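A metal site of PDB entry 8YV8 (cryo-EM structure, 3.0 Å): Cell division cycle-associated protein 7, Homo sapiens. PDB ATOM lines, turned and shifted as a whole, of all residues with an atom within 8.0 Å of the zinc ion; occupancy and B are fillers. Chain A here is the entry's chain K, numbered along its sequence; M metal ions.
Four residues have an atom within 4 Å of the zinc ion: His 8, Cys 64, Cys 66 and Cys 69. The nearest printed residue that does not touch the zinc ion is Pro 59 (4.3 Å).
SG of Cys 66 sits close to N of Phe 68 (3.4 Å). O of Pro 58 lies within hydrogen-bond range of N of Cys 64, 3.2 Å away.
The zinc ion is bound by a ring nitrogen (NE2) of His 8, at 2.0 Å. The side-chain sulfur (SG) of Cys 66 binds the zinc ion. The zinc ion is bound by SG of Cys 69 (2.3 Å). The side-chain sulfur (SG) of Cys 64 binds the zinc ion (2.4 Å).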
ATOM      1  N   HIS A   8      22.990  25.466 -27.698  1.00  0.00           N
ATOM      2  CA  HIS A   8      24.123  25.898 -26.882  1.00  0.00           C
ATOM      3  C   HIS A   8      23.961  25.453 -25.438  1.00  0.00           C
ATOM      4  O   HIS A   8      24.931  24.997 -24.809  1.00  0.00           O
ATOM      5  CB  HIS A   8      24.267  27.424 -26.963  1.00  0.00           C
ATOM      6  CG  HIS A   8      25.272  27.992 -26.011  1.00  0.00           C
ATOM      7  ND1 HIS A   8      26.629  28.005 -26.283  1.00  0.00           N
ATOM      8  CD2 HIS A   8      25.129  28.565 -24.797  1.00  0.00           C
ATOM      9  CE1 HIS A   8      27.269  28.558 -25.273  1.00  0.00           C
ATOM     10  NE2 HIS A   8      26.383  28.917 -24.359  1.00  0.00           N
ATOM     11  N   GLN A   9      22.749  25.561 -24.886  1.00  0.00           N
ATOM     12  CA  GLN A   9      22.536  25.198 -23.486  1.00  0.00           C
ATOM     13  C   GLN A   9      22.604  23.692 -23.281  1.00  0.00           C
ATOM     14  O   GLN A   9      23.304  23.201 -22.396  1.00  0.00           O
ATOM     15  CB  GLN A   9      21.196  25.743 -23.008  1.00  0.00           C
ATOM     16  N   ARG A  11      23.432  21.282 -25.706  1.00  0.00           N
ATOM     17  CA  ARG A  11      24.594  20.720 -26.397  1.00  0.00           C
ATOM     18  C   ARG A  11      24.329  19.317 -26.922  1.00  0.00           C
ATOM     19  O   ARG A  11      25.225  18.461 -26.923  1.00  0.00           O
ATOM     20  CB  ARG A  11      25.828  20.765 -25.498  1.00  0.00           C
ATOM     21  CG  ARG A  11      27.158  20.759 -26.219  1.00  0.00           C
ATOM     22  CD  ARG A  11      28.299  21.118 -25.288  1.00  0.00           C
ATOM     23  NE  ARG A  11      27.825  21.772 -24.068  1.00  0.00           N
ATOM     24  CZ  ARG A  11      27.894  21.229 -22.860  1.00  0.00           C
ATOM     25  NH1 ARG A  11      28.406  20.029 -22.664  1.00  0.00           N
ATOM     26  NH2 ARG A  11      27.433  21.925 -21.821  1.00  0.00           N
ATOM     27  N   ARG A  30      27.171  29.918 -30.813  1.00  0.00           N
ATOM     28  CA  ARG A  30      26.625  30.172 -29.492  1.00  0.00           C
ATOM     29  C   ARG A  30      25.343  30.999 -29.501  1.00  0.00           C
ATOM     30  O   ARG A  30      24.705  31.136 -28.452  1.00  0.00           O
ATOM     31  CB  ARG A  30      27.685  30.862 -28.619  1.00  0.00           C
ATOM     32  CG  ARG A  30      28.124  32.226 -29.133  1.00  0.00           C
ATOM     33  CD  ARG A  30      27.444  33.369 -28.384  1.00  0.00           C
ATOM     34  NE  ARG A  30      27.911  34.666 -28.856  1.00  0.00           N
ATOM     35  CZ  ARG A  30      27.386  35.829 -28.496  1.00  0.00           C
ATOM     36  NH1 ARG A  30      26.360  35.899 -27.669  1.00  0.00           N
ATOM     37  NH2 ARG A  30      27.905  36.960 -28.970  1.00  0.00           N
ATOM     38  N   PHE A  33      19.886  28.419 -29.810  1.00  0.00           N
ATOM     39  CA  PHE A  33      19.297  27.777 -28.651  1.00  0.00           C
ATOM     40  C   PHE A  33      18.050  27.016 -29.062  1.00  0.00           C
ATOM     41  O   PHE A  33      17.350  27.422 -29.994  1.00  0.00           O
ATOM     42  CB  PHE A  33      18.943  28.783 -27.559  1.00  0.00           C
ATOM     43  CG  PHE A  33      20.085  29.151 -26.668  1.00  0.00           C
ATOM     44  CD1 PHE A  33      21.045  30.055 -27.090  1.00  0.00           C
ATOM     45  CD2 PHE A  33      20.208  28.595 -25.402  1.00  0.00           C
ATOM     46  CE1 PHE A  33      22.101  30.397 -26.278  1.00  0.00           C
ATOM     47  CE2 PHE A  33      21.259  28.929 -24.587  1.00  0.00           C
ATOM     48  CZ  PHE A  33      22.212  29.835 -25.016  1.00  0.00           C
ATOM     49  N   TYR A  42      14.441  30.869 -19.295  1.00  0.00           N
ATOM     50  CA  TYR A  42      14.165  32.295 -19.244  1.00  0.00           C
ATOM     51  C   TYR A  42      12.724  32.664 -19.581  1.00  0.00           C
ATOM     52  O   TYR A  42      12.407  33.862 -19.612  1.00  0.00           O
ATOM     53  CB  TYR A  42      15.114  33.054 -20.171  1.00  0.00           C
ATOM     54  CG  TYR A  42      16.548  32.597 -20.082  1.00  0.00           C
ATOM     55  CD1 TYR A  42      17.331  32.919 -18.980  1.00  0.00           C
ATOM     56  CD2 TYR A  42      17.123  31.833 -21.089  1.00  0.00           C
ATOM     57  CE1 TYR A  42      18.643  32.508 -18.891  1.00  0.00           C
ATOM     58  CE2 TYR A  42      18.434  31.409 -21.003  1.00  0.00           C
ATOM     59  CZ  TYR A  42      19.194  31.746 -19.904  1.00  0.00           C
ATOM     60  OH  TYR A  42      20.493  31.330 -19.819  1.00  0.00           O
ATOM     61  N   PRO A  58      21.014  34.636 -25.342  1.00  0.00           N
ATOM     62  CA  PRO A  58      21.256  34.888 -23.908  1.00  0.00           C
ATOM     63  C   PRO A  58      22.716  35.171 -23.593  1.00  0.00           C
ATOM     64  O   PRO A  58      22.995  35.973 -22.690  1.00  0.00           O
ATOM     65  CB  PRO A  58      20.762  33.594 -23.230  1.00  0.00           C
ATOM     66  CG  PRO A  58      20.294  32.681 -24.342  1.00  0.00           C
ATOM     67  CD  PRO A  58      20.096  33.517 -25.559  1.00  0.00           C
ATOM     68  N   PRO A  59      23.680  34.542 -24.281  1.00  0.00           N
ATOM     69  CA  PRO A  59      25.065  35.008 -24.117  1.00  0.00           C
ATOM     70  C   PRO A  59      25.275  36.471 -24.508  1.00  0.00           C
ATOM     71  O   PRO A  59      26.121  37.142 -23.910  1.00  0.00           O
ATOM     72  CB  PRO A  59      25.874  34.064 -25.009  1.00  0.00           C
ATOM     73  CG  PRO A  59      25.070  32.835 -25.053  1.00  0.00           C
ATOM     74  CD  PRO A  59      23.649  33.287 -25.044  1.00  0.00           C
ATOM     75  N   ILE A  63      23.110  36.822 -19.955  1.00  0.00           N
ATOM     76  CA  ILE A  63      22.257  36.064 -19.047  1.00  0.00           C
ATOM     77  C   ILE A  63      22.350  34.561 -19.305  1.00  0.00           C
ATOM     78  O   ILE A  63      21.566  33.789 -18.739  1.00  0.00           O
ATOM     79  CB  ILE A  63      20.804  36.546 -19.113  1.00  0.00           C
ATOM     80  CG1 ILE A  63      20.175  36.175 -20.465  1.00  0.00           C
ATOM     81  CG2 ILE A  63      20.723  38.048 -18.894  1.00  0.00           C
ATOM     82  CD1 ILE A  63      18.711  36.520 -20.565  1.00  0.00           C
ATOM     83  N   CYS A  64      23.279  34.123 -20.152  1.00  0.00           N
ATOM     84  CA  CYS A  64      23.460  32.704 -20.404  1.00  0.00           C
ATOM     85  C   CYS A  64      23.920  31.987 -19.140  1.00  0.00           C
ATOM     86  O   CYS A  64      24.823  32.465 -18.446  1.00  0.00           O
ATOM     87  CB  CYS A  64      24.466  32.478 -21.536  1.00  0.00           C
ATOM     88  SG  CYS A  64      24.734  30.746 -22.009  1.00  0.00           S
ATOM     89  N   ASN A  65      23.293  30.858 -18.842  1.00  0.00           N
ATOM     90  CA  ASN A  65      23.651  30.050 -17.685  1.00  0.00           C
ATOM     91  C   ASN A  65      24.109  28.662 -18.103  1.00  0.00           C
ATOM     92  O   ASN A  65      23.994  27.694 -17.343  1.00  0.00           O
ATOM     93  CB  ASN A  65      22.494  29.961 -16.689  1.00  0.00           C
ATOM     94  CG  ASN A  65      21.176  29.620 -17.356  1.00  0.00           C
ATOM     95  OD1 ASN A  65      21.138  28.968 -18.392  1.00  0.00           O
ATOM     96  ND2 ASN A  65      20.084  30.083 -16.752  1.00  0.00           N
ATOM     97  N   CYS A  66      24.627  28.534 -19.328  1.00  0.00           N
ATOM     98  CA  CYS A  66      25.211  27.283 -19.763  1.00  0.00           C
ATOM     99  C   CYS A  66      26.457  26.975 -18.941  1.00  0.00           C
ATOM    100  O   CYS A  66      27.149  27.871 -18.468  1.00  0.00           O
ATOM    101  CB  CYS A  66      25.564  27.342 -21.250  1.00  0.00           C
ATOM    102  SG  CYS A  66      27.261  27.858 -21.571  1.00  0.00           S
ATOM    103  N   SER A  67      26.741  25.683 -18.790  1.00  0.00           N
ATOM    104  CA  SER A  67      27.859  25.262 -17.959  1.00  0.00           C
ATOM    105  C   SER A  67      29.181  25.796 -18.495  1.00  0.00           C
ATOM    106  O   SER A  67      30.064  26.179 -17.721  1.00  0.00           O
ATOM    107  CB  SER A  67      27.903  23.741 -17.858  1.00  0.00           C
ATOM    108  OG  SER A  67      26.815  23.275 -17.081  1.00  0.00           O
ATOM    109  N   PHE A  68      29.338  25.829 -19.820  1.00  0.00           N
ATOM    110  CA  PHE A  68      30.543  26.412 -20.404  1.00  0.00           C
ATOM    111  C   PHE A  68      30.667  27.886 -20.035  1.00  0.00           C
ATOM    112  O   PHE A  68      31.691  28.317 -19.491  1.00  0.00           O
ATOM    113  CB  PHE A  68      30.519  26.220 -21.915  1.00  0.00           C
ATOM    114  CG  PHE A  68      31.579  26.996 -22.652  1.00  0.00           C
ATOM    115  CD1 PHE A  68      32.915  26.897 -22.281  1.00  0.00           C
ATOM    116  CD2 PHE A  68      31.243  27.814 -23.718  1.00  0.00           C
ATOM    117  CE1 PHE A  68      33.883  27.607 -22.961  1.00  0.00           C
ATOM    118  CE2 PHE A  68      32.205  28.531 -24.392  1.00  0.00           C
ATOM    119  CZ  PHE A  68      33.536  28.424 -24.018  1.00  0.00           C
ATOM    120  N   CYS A  69      29.611  28.667 -20.291  1.00  0.00           N
ATOM    121  CA  CYS A  69      29.632  30.085 -19.950  1.00  0.00           C
ATOM    122  C   CYS A  69      29.686  30.283 -18.437  1.00  0.00           C
ATOM    123  O   CYS A  69      30.344  31.206 -17.954  1.00  0.00           O
ATOM    124  CB  CYS A  69      28.422  30.787 -20.551  1.00  0.00           C
ATOM    125  SG  CYS A  69      28.593  31.213 -22.298  1.00  0.00           S
ATOM    126  N   ARG A  70      28.988  29.427 -17.680  1.00  0.00           N
ATOM    127  CA  ARG A  70      29.016  29.537 -16.232  1.00  0.00           C
ATOM    128  C   ARG A  70      30.420  29.323 -15.687  1.00  0.00           C
ATOM    129  O   ARG A  70      30.812  29.961 -14.705  1.00  0.00           O
ATOM    130  CB  ARG A  70      28.038  28.531 -15.622  1.00  0.00           C
ATOM    131  CG  ARG A  70      26.631  29.087 -15.410  1.00  0.00           C
ATOM    132  CD  ARG A  70      26.487  29.852 -14.111  1.00  0.00           C
ATOM    133  NE  ARG A  70      26.417  28.947 -12.980  1.00  0.00           N
ATOM    134  CZ  ARG A  70      26.737  29.274 -11.725  1.00  0.00           C
ATOM    135  NH1 ARG A  70      27.194  30.470 -11.424  1.00  0.00           N
ATOM    136  NH2 ARG A  70      26.604  28.362 -10.772  1.00  0.00           N
ATOM    137  N   GLN A  71      31.186  28.429 -16.320  1.00  0.00           N
ATOM    138  CA  GLN A  71      32.582  28.231 -15.931  1.00  0.00           C
ATOM    139  C   GLN A  71      33.452  29.391 -16.391  1.00  0.00           C
ATOM    140  O   GLN A  71      34.422  29.762 -15.714  1.00  0.00           O
ATOM    141  CB  GLN A  71      33.093  26.913 -16.492  1.00  0.00           C
ATOM    142  CG  GLN A  71      32.928  25.731 -15.556  1.00  0.00           C
ATOM    143  CD  GLN A  71      32.511  24.467 -16.283  1.00  0.00           C
ATOM    144  OE1 GLN A  71      32.475  24.429 -17.514  1.00  0.00           O
ATOM    145  NE2 GLN A  71      32.173  23.434 -15.526  1.00  0.00           N
ATOM    146  N   ARG A  72      33.137  29.983 -17.555  1.00  0.00           N
ATOM    147  CA  ARG A  72      33.875  31.166 -17.999  1.00  0.00           C
ATOM    148  C   ARG A  72      33.713  32.317 -17.010  1.00  0.00           C
ATOM    149  O   ARG A  72      34.596  33.173 -16.917  1.00  0.00           O
ATOM    150  CB  ARG A  72      33.422  31.604 -19.386  1.00  0.00           C
ATOM    151  CG  ARG A  72      33.575  30.541 -20.457  1.00  0.00           C
ATOM    152  CD  ARG A  72      33.018  31.037 -21.791  1.00  0.00           C
ATOM    153  NE  ARG A  72      33.892  32.010 -22.436  1.00  0.00           N
ATOM    154  CZ  ARG A  72      35.113  31.748 -22.906  1.00  0.00           C
ATOM    155  NH1 ARG A  72      35.639  30.541 -22.822  1.00  0.00           N
ATOM    156  NH2 ARG A  72      35.806  32.731 -23.464  1.00  0.00           N
ATOM    157  N   ASP A  73      32.603  32.361 -16.292  1.00  0.00           N
ATOM    158  CA  ASP A  73      32.405  33.375 -15.259  1.00  0.00           C
ATOM    159  C   ASP A  73      33.154  33.071 -13.977  1.00  0.00           C
ATOM    160  O   ASP A  73      33.138  33.893 -13.060  1.00  0.00           O
ATOM    161  CB  ASP A  73      30.907  33.526 -14.958  1.00  0.00           C
ATOM    162  CG  ASP A  73      30.074  33.683 -16.209  1.00  0.00           C
ATOM    163  OD1 ASP A  73      30.583  34.245 -17.202  1.00  0.00           O
ATOM    164  OD2 ASP A  73      28.902  33.241 -16.205  1.00  0.00           O
HETATM  165 ZN    ZN M   1      26.833  29.788 -22.591  1.00  0.00          ZN
